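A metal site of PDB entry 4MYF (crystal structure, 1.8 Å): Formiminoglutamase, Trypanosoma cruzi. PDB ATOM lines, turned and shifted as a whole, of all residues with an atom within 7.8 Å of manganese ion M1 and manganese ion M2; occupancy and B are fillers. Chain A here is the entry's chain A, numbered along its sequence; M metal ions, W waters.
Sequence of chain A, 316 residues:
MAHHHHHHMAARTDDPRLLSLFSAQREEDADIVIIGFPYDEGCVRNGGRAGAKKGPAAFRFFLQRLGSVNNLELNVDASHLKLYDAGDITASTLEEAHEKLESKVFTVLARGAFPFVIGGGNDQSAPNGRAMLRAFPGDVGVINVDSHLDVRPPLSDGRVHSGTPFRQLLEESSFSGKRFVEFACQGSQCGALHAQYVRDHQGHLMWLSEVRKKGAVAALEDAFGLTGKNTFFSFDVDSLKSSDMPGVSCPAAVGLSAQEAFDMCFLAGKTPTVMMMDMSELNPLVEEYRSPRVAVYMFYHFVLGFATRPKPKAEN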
ATOM      1  N   GLY A  42      24.541  23.822  14.820  1.00  0.00           N
ATOM      2  CA  GLY A  42      23.530  23.050  14.104  1.00  0.00           C
ATOM      3  C   GLY A  42      22.570  24.010  13.417  1.00  0.00           C
ATOM      4  O   GLY A  42      23.000  24.844  12.623  1.00  0.00           O
ATOM      5  N   CYS A  43      21.286  23.907  13.740  1.00  0.00           N
ATOM      6  CA  CYS A  43      20.286  24.745  13.073  1.00  0.00           C
ATOM      7  C   CYS A  43      20.383  26.243  13.404  1.00  0.00           C
ATOM      8  O   CYS A  43      19.767  27.062  12.718  1.00  0.00           O
ATOM      9  CB  CYS A  43      18.861  24.231  13.342  1.00  0.00           C
ATOM     10  SG  CYS A  43      17.627  24.875  12.197  1.00  0.00           S
ATOM     11  N   ASN A  46      21.200  28.022  10.452  1.00  0.00           N
ATOM     12  CA  ASN A  46      20.112  28.121   9.485  1.00  0.00           C
ATOM     13  C   ASN A  46      18.978  28.990   9.998  1.00  0.00           C
ATOM     14  O   ASN A  46      17.806  28.639   9.878  1.00  0.00           O
ATOM     15  CB  ASN A  46      19.580  26.727   9.128  1.00  0.00           C
ATOM     16  CG  ASN A  46      20.646  25.820   8.552  1.00  0.00           C
ATOM     17  OD1 ASN A  46      21.823  26.194   8.444  1.00  0.00           O
ATOM     18  ND2 ASN A  46      20.242  24.612   8.158  1.00  0.00           N
ATOM     19  N   GLY A 121      23.640  21.048  19.327  1.00  0.00           N
ATOM     20  CA  GLY A 121      23.174  21.164  17.957  1.00  0.00           C
ATOM     21  C   GLY A 121      23.422  19.938  17.064  1.00  0.00           C
ATOM     22  O   GLY A 121      24.165  19.019  17.456  1.00  0.00           O
ATOM     23  N   ASN A 122      22.793  19.951  15.885  1.00  0.00           N
ATOM     24  CA  ASN A 122      22.871  18.892  14.869  1.00  0.00           C
ATOM     25  C   ASN A 122      24.278  18.430  14.523  1.00  0.00           C
ATOM     26  O   ASN A 122      24.477  17.287  14.088  1.00  0.00           O
ATOM     27  CB  ASN A 122      22.294  19.362  13.528  1.00  0.00           C
ATOM     28  CG  ASN A 122      20.795  19.529  13.547  1.00  0.00           C
ATOM     29  OD1 ASN A 122      20.048  18.647  14.006  1.00  0.00           O
ATOM     30  ND2 ASN A 122      20.333  20.638  12.970  1.00  0.00           N
ATOM     31  N   ASP A 123      25.241  19.332  14.644  1.00  0.00           N
ATOM     32  CA  ASP A 123      26.599  19.023  14.187  1.00  0.00           C
ATOM     33  C   ASP A 123      27.196  17.812  14.901  1.00  0.00           C
ATOM     34  O   ASP A 123      28.095  17.155  14.380  1.00  0.00           O
ATOM     35  CB  ASP A 123      27.507  20.253  14.281  1.00  0.00           C
ATOM     36  CG  ASP A 123      27.216  21.282  13.192  1.00  0.00           C
ATOM     37  OD1 ASP A 123      26.226  21.097  12.452  1.00  0.00           O
ATOM     38  OD2 ASP A 123      27.975  22.266  13.062  1.00  0.00           O
ATOM     39  N   SER A 125      26.058  14.966  15.119  1.00  0.00           N
ATOM     40  CA  SER A 125      25.732  13.719  14.444  1.00  0.00           C
ATOM     41  C   SER A 125      26.836  13.264  13.476  1.00  0.00           C
ATOM     42  O   SER A 125      26.909  12.091  13.143  1.00  0.00           O
ATOM     43  CB  SER A 125      24.404  13.844  13.682  1.00  0.00           C
ATOM     44  OG  SER A 125      23.375  14.284  14.540  1.00  0.00           O
ATOM     45  N   ASN A 144      18.014  10.058   9.761  1.00  0.00           N
ATOM     46  CA  ASN A 144      17.953  11.403  10.292  1.00  0.00           C
ATOM     47  C   ASN A 144      16.485  11.826  10.381  1.00  0.00           C
ATOM     48  O   ASN A 144      15.846  12.098   9.345  1.00  0.00           O
ATOM     49  CB  ASN A 144      18.723  12.393   9.413  1.00  0.00           C
ATOM     50  CG  ASN A 144      18.622  13.833   9.916  1.00  0.00           C
ATOM     51  OD1 ASN A 144      18.490  14.057  11.124  1.00  0.00           O
ATOM     52  ND2 ASN A 144      18.693  14.787   9.000  1.00  0.00           N
ATOM     53  N   VAL A 145      15.968  11.872  11.605  1.00  0.00           N
ATOM     54  CA  VAL A 145      14.617  12.326  11.869  1.00  0.00           C
ATOM     55  C   VAL A 145      14.753  13.839  12.035  1.00  0.00           C
ATOM     56  O   VAL A 145      15.363  14.290  13.005  1.00  0.00           O
ATOM     57  CB  VAL A 145      14.033  11.696  13.153  1.00  0.00           C
ATOM     58  CG1 VAL A 145      12.639  12.271  13.455  1.00  0.00           C
ATOM     59  CG2 VAL A 145      13.964  10.171  13.048  1.00  0.00           C
ATOM     60  N   ASP A 146      14.236  14.588  11.075  1.00  0.00           N
ATOM     61  CA  ASP A 146      14.527  16.006  10.995  1.00  0.00           C
ATOM     62  C   ASP A 146      13.551  16.694  10.040  1.00  0.00           C
ATOM     63  O   ASP A 146      13.254  16.174   8.967  1.00  0.00           O
ATOM     64  CB  ASP A 146      15.955  16.185  10.479  1.00  0.00           C
ATOM     65  CG  ASP A 146      16.506  17.587  10.700  1.00  0.00           C
ATOM     66  OD1 ASP A 146      15.730  18.516  11.012  1.00  0.00           O
ATOM     67  OD2 ASP A 146      17.730  17.742  10.538  1.00  0.00           O
ATOM     68  N   SER A 147      13.032  17.852  10.441  1.00  0.00           N
ATOM     69  CA  SER A 147      12.189  18.605   9.507  1.00  0.00           C
ATOM     70  C   SER A 147      13.051  19.142   8.357  1.00  0.00           C
ATOM     71  O   SER A 147      12.543  19.413   7.285  1.00  0.00           O
ATOM     72  CB  SER A 147      11.433  19.726  10.208  1.00  0.00           C
ATOM     73  OG  SER A 147      12.322  20.657  10.790  1.00  0.00           O
ATOM     74  N   HIS A 148      14.370  19.255   8.589  1.00  0.00           N
ATOM     75  CA  HIS A 148      15.336  19.763   7.594  1.00  0.00           C
ATOM     76  C   HIS A 148      16.221  18.630   7.041  1.00  0.00           C
ATOM     77  O   HIS A 148      16.379  17.604   7.690  1.00  0.00           O
ATOM     78  CB  HIS A 148      16.245  20.812   8.243  1.00  0.00           C
ATOM     79  CG  HIS A 148      15.534  21.824   9.093  1.00  0.00           C
ATOM     80  ND1 HIS A 148      15.333  21.669  10.440  1.00  0.00           N
ATOM     81  CD2 HIS A 148      14.987  23.025   8.763  1.00  0.00           C
ATOM     82  CE1 HIS A 148      14.680  22.708  10.924  1.00  0.00           C
ATOM     83  NE2 HIS A 148      14.467  23.554   9.923  1.00  0.00           N
ATOM     84  N   LEU A 149      16.825  18.811   5.857  1.00  0.00           N
ATOM     85  CA  LEU A 149      17.710  17.752   5.314  1.00  0.00           C
ATOM     86  C   LEU A 149      19.128  17.651   5.913  1.00  0.00           C
ATOM     87  O   LEU A 149      19.747  16.567   5.908  1.00  0.00           O
ATOM     88  CB  LEU A 149      17.802  17.837   3.783  1.00  0.00           C
ATOM     89  CG  LEU A 149      16.633  17.312   2.953  1.00  0.00           C
ATOM     90  CD1 LEU A 149      17.087  17.213   1.516  1.00  0.00           C
ATOM     91  CD2 LEU A 149      16.163  15.955   3.438  1.00  0.00           C
ATOM     92  N   ASP A 150      19.636  18.775   6.403  1.00  0.00           N
ATOM     93  CA  ASP A 150      20.992  18.839   6.989  1.00  0.00           C
ATOM     94  C   ASP A 150      22.084  18.358   6.031  1.00  0.00           C
ATOM     95  O   ASP A 150      22.916  17.517   6.402  1.00  0.00           O
ATOM     96  CB  ASP A 150      21.058  18.015   8.281  1.00  0.00           C
ATOM     97  CG  ASP A 150      20.501  18.737   9.482  1.00  0.00           C
ATOM     98  OD1 ASP A 150      19.745  19.727   9.306  1.00  0.00           O
ATOM     99  OD2 ASP A 150      20.805  18.296  10.619  1.00  0.00           O
ATOM    100  N   PRO A 165      26.071  17.800   9.061  1.00  0.00           N
ATOM    101  CA  PRO A 165      26.526  16.490   9.523  1.00  0.00           C
ATOM    102  C   PRO A 165      26.220  15.338   8.553  1.00  0.00           C
ATOM    103  O   PRO A 165      27.023  14.401   8.457  1.00  0.00           O
ATOM    104  CB  PRO A 165      25.762  16.304  10.842  1.00  0.00           C
ATOM    105  CG  PRO A 165      24.560  17.221  10.739  1.00  0.00           C
ATOM    106  CD  PRO A 165      25.086  18.409   9.967  1.00  0.00           C
ATOM    107  N   PHE A 166      25.107  15.390   7.828  1.00  0.00           N
ATOM    108  CA  PHE A 166      24.797  14.269   6.941  1.00  0.00           C
ATOM    109  C   PHE A 166      25.378  14.377   5.539  1.00  0.00           C
ATOM    110  O   PHE A 166      25.456  13.391   4.805  1.00  0.00           O
ATOM    111  CB  PHE A 166      23.291  13.945   6.966  1.00  0.00           C
ATOM    112  CG  PHE A 166      22.816  13.638   8.350  1.00  0.00           C
ATOM    113  CD1 PHE A 166      23.070  12.404   8.922  1.00  0.00           C
ATOM    114  CD2 PHE A 166      22.200  14.608   9.115  1.00  0.00           C
ATOM    115  CE1 PHE A 166      22.685  12.121  10.226  1.00  0.00           C
ATOM    116  CE2 PHE A 166      21.807  14.327  10.424  1.00  0.00           C
ATOM    117  CZ  PHE A 166      22.033  13.085  10.972  1.00  0.00           C
ATOM    118  N   GLU A 182      16.138  10.119   5.281  1.00  0.00           N
ATOM    119  CA  GLU A 182      15.714  11.398   5.819  1.00  0.00           C
ATOM    120  C   GLU A 182      14.237  11.223   6.165  1.00  0.00           C
ATOM    121  O   GLU A 182      13.413  10.991   5.282  1.00  0.00           O
ATOM    122  CB  GLU A 182      15.890  12.503   4.775  1.00  0.00           C
ATOM    123  CG  GLU A 182      17.333  12.718   4.312  1.00  0.00           C
ATOM    124  CD  GLU A 182      18.089  13.730   5.162  1.00  0.00           C
ATOM    125  OE1 GLU A 182      17.732  13.944   6.349  1.00  0.00           O
ATOM    126  OE2 GLU A 182      19.058  14.323   4.635  1.00  0.00           O
ATOM    127  N   GLN A 189      10.764  23.336   3.574  1.00  0.00           N
ATOM    128  CA  GLN A 189      12.068  23.594   4.195  1.00  0.00           C
ATOM    129  C   GLN A 189      13.216  22.838   3.554  1.00  0.00           C
ATOM    130  O   GLN A 189      14.272  22.701   4.173  1.00  0.00           O
ATOM    131  CB  GLN A 189      12.043  23.132   5.651  1.00  0.00           C
ATOM    132  CG  GLN A 189      11.130  23.898   6.556  1.00  0.00           C
ATOM    133  CD  GLN A 189      11.643  23.834   7.966  1.00  0.00           C
ATOM    134  OE1 GLN A 189      11.801  24.861   8.623  1.00  0.00           O
ATOM    135  NE2 GLN A 189      11.943  22.617   8.427  1.00  0.00           N
ATOM    136  N   SER A 234      19.056   8.955  14.636  1.00  0.00           N
ATOM    137  CA  SER A 234      19.432  10.356  14.920  1.00  0.00           C
ATOM    138  C   SER A 234      18.180  11.229  14.934  1.00  0.00           C
ATOM    139  O   SER A 234      17.531  11.416  13.896  1.00  0.00           O
ATOM    140  CB  SER A 234      20.416  10.856  13.858  1.00  0.00           C
ATOM    141  OG  SER A 234      20.994  12.105  14.211  1.00  0.00           O
ATOM    142  N   PHE A 235      17.842  11.777  16.098  1.00  0.00           N
ATOM    143  CA  PHE A 235      16.551  12.419  16.283  1.00  0.00           C
ATOM    144  C   PHE A 235      16.719  13.911  16.556  1.00  0.00           C
ATOM    145  O   PHE A 235      17.003  14.297  17.684  1.00  0.00           O
ATOM    146  CB  PHE A 235      15.786  11.762  17.446  1.00  0.00           C
ATOM    147  CG  PHE A 235      14.278  11.788  17.279  1.00  0.00           C
ATOM    148  CD1 PHE A 235      13.644  12.941  16.857  1.00  0.00           C
ATOM    149  CD2 PHE A 235      13.516  10.649  17.550  1.00  0.00           C
ATOM    150  CE1 PHE A 235      12.259  12.967  16.699  1.00  0.00           C
ATOM    151  CE2 PHE A 235      12.127  10.684  17.402  1.00  0.00           C
ATOM    152  CZ  PHE A 235      11.501  11.835  16.976  1.00  0.00           C
ATOM    153  N   ASP A 236      16.563  14.729  15.524  1.00  0.00           N
ATOM    154  CA  ASP A 236      16.533  16.181  15.670  1.00  0.00           C
ATOM    155  C   ASP A 236      15.136  16.564  16.151  1.00  0.00           C
ATOM    156  O   ASP A 236      14.164  16.372  15.425  1.00  0.00           O
ATOM    157  CB  ASP A 236      16.855  16.848  14.322  1.00  0.00           C
ATOM    158  CG  ASP A 236      16.832  18.374  14.367  1.00  0.00           C
ATOM    159  OD1 ASP A 236      16.299  18.967  15.312  1.00  0.00           O
ATOM    160  OD2 ASP A 236      17.335  18.996  13.419  1.00  0.00           O
ATOM    161  N   VAL A 237      15.039  17.071  17.384  1.00  0.00           N
ATOM    162  CA  VAL A 237      13.722  17.320  17.979  1.00  0.00           C
ATOM    163  C   VAL A 237      12.950  18.489  17.348  1.00  0.00           C
ATOM    164  O   VAL A 237      11.772  18.698  17.667  1.00  0.00           O
ATOM    165  CB  VAL A 237      13.761  17.470  19.540  1.00  0.00           C
ATOM    166  CG1 VAL A 237      14.140  16.138  20.188  1.00  0.00           C
ATOM    167  CG2 VAL A 237      14.712  18.581  19.967  1.00  0.00           C
ATOM    168  N   ASP A 238      13.592  19.256  16.461  1.00  0.00           N
ATOM    169  CA  ASP A 238      12.824  20.253  15.722  1.00  0.00           C
ATOM    170  C   ASP A 238      12.014  19.585  14.612  1.00  0.00           C
ATOM    171  O   ASP A 238      11.391  20.257  13.789  1.00  0.00           O
ATOM    172  CB  ASP A 238      13.714  21.415  15.232  1.00  0.00           C
ATOM    173  CG  ASP A 238      14.623  21.038  14.074  1.00  0.00           C
ATOM    174  OD1 ASP A 238      14.322  20.077  13.322  1.00  0.00           O
ATOM    175  OD2 ASP A 238      15.644  21.747  13.901  1.00  0.00           O
ATOM    176  N   SER A 239      12.010  18.250  14.605  1.00  0.00           N
ATOM    177  CA  SER A 239      11.107  17.515  13.731  1.00  0.00           C
ATOM    178  C   SER A 239       9.709  17.447  14.358  1.00  0.00           C
ATOM    179  O   SER A 239       8.740  17.084  13.690  1.00  0.00           O
ATOM    180  CB  SER A 239      11.615  16.093  13.464  1.00  0.00           C
ATOM    181  OG  SER A 239      11.704  15.343  14.660  1.00  0.00           O
ATOM    182  N   VAL A 248      13.256  24.554  20.799  1.00  0.00           N
ATOM    183  CA  VAL A 248      14.271  24.074  19.870  1.00  0.00           C
ATOM    184  C   VAL A 248      14.808  25.288  19.129  1.00  0.00           C
ATOM    185  O   VAL A 248      14.176  26.346  19.103  1.00  0.00           O
ATOM    186  CB  VAL A 248      13.720  23.048  18.851  1.00  0.00           C
ATOM    187  CG1 VAL A 248      13.143  21.838  19.582  1.00  0.00           C
ATOM    188  CG2 VAL A 248      12.696  23.704  17.928  1.00  0.00           C
ATOM    189  N   CYS A 250      15.114  25.895  15.975  1.00  0.00           N
ATOM    190  CA  CYS A 250      14.308  26.200  14.795  1.00  0.00           C
ATOM    191  C   CYS A 250      12.912  25.581  14.909  1.00  0.00           C
ATOM    192  O   CYS A 250      12.658  24.508  14.371  1.00  0.00           O
ATOM    193  CB  CYS A 250      14.993  25.627  13.551  1.00  0.00           C
ATOM    194  SG  CYS A 250      16.649  26.304  13.269  1.00  0.00           S
ATOM    195  N   SER A 280      19.177  15.932  19.016  1.00  0.00           N
ATOM    196  CA  SER A 280      19.778  17.234  18.765  1.00  0.00           C
ATOM    197  C   SER A 280      18.753  18.351  18.808  1.00  0.00           C
ATOM    198  O   SER A 280      17.569  18.119  18.617  1.00  0.00           O
ATOM    199  CB  SER A 280      20.458  17.254  17.388  1.00  0.00           C
ATOM    200  OG  SER A 280      21.529  16.317  17.331  1.00  0.00           O
ATOM    201  N   GLU A 281      19.247  19.562  19.050  1.00  0.00           N
ATOM    202  CA  GLU A 281      18.519  20.830  18.911  1.00  0.00           C
ATOM    203  C   GLU A 281      17.642  21.256  20.085  1.00  0.00           C
ATOM    204  O   GLU A 281      16.938  22.268  19.992  1.00  0.00           O
ATOM    205  CB  GLU A 281      17.754  20.890  17.575  1.00  0.00           C
ATOM    206  CG  GLU A 281      18.657  20.802  16.326  1.00  0.00           C
ATOM    207  CD  GLU A 281      19.589  21.993  16.187  1.00  0.00           C
ATOM    208  OE1 GLU A 281      19.186  23.113  16.581  1.00  0.00           O
ATOM    209  OE2 GLU A 281      20.718  21.826  15.661  1.00  0.00           O
HETATM  210 MN    MN M   1      16.231  20.369  12.073  1.00  0.00          MN
HETATM  211 MN    MN M   2      18.941  18.788  11.990  1.00  0.00          MN
HETATM  212  O   HOH W   1      18.298  20.778  11.181  1.00  0.00           O
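The backbone carbonyl oxygen (O) of Asp 236 is in hydrogen-bond range of the side-chain hydroxyl (OG) of Ser 239 (2.8 Å). The backbone carbonyl oxygen of Val 145 lies within hydrogen-bond range of the backbone NH of Asp 236, at 2.8 Å. OD2 of Asp 146 lies close to ND2 of Asn 144 (3.5 Å). The side-chain hydroxyl (OG) of Ser 147 sits close to a ring nitrogen (ND1) of His 148, 3.2 Å away. The backbone NH of Asn 122 lies within hydrogen-bond range of the side-chain carboxylate of Glu 281, 2.8 Å away. The backbone carbonyl oxygen of Asn 122 sits at hydrogen-bond distance from the side-chain hydroxyl of Ser 125 (3.2 Å). N of Phe 166 is in hydrogen-bond range of O of Asp 150 (3.4 Å). The side-chain sulfur (SG) of Cys 250 forms a disulfide with the side-chain sulfur (SG) of Cys 43, at 2.0 Å.
Four residues have an atom within 4 Å of manganese ion M1: Asp 146, His 148, Asp 236 and Asp 238.
Within 4 Å of manganese ion M2: Asn 122, Asp 146, Asp 150 and Asp 236.
OD1 of Asp 146 is bound to manganese ion M1. Manganese ion M1 is bound by the side-chain carboxylate (OD2) of Asp 236, 2.2 Å away. A ring nitrogen (ND1) of His 148 is bound to manganese ion M1, at 2.3 Å. Manganese ion M1 is bound by water W1 (2.3 Å). Manganese ion M1 is bound by OD1 of Asp 238 (2.3 Å). The side-chain carboxylate (OD2) of Asp 238 is bound to manganese ion M1, 2.4 Å away. Manganese ion M1 has six donor atoms within binding distance.
Manganese ion M2 is bound by the side-chain carboxylate of Asp 236 (2.2 Å), the side-chain carboxylate of Asp 146 (2.2 Å), water W1 (2.2 Å), the side-chain amide oxygen of Asn 122 (2.3 Å), the side-chain carboxylate of Asp 150 (2.4 Å) and the side-chain amide nitrogen of Asn 122 (2.5 Å).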
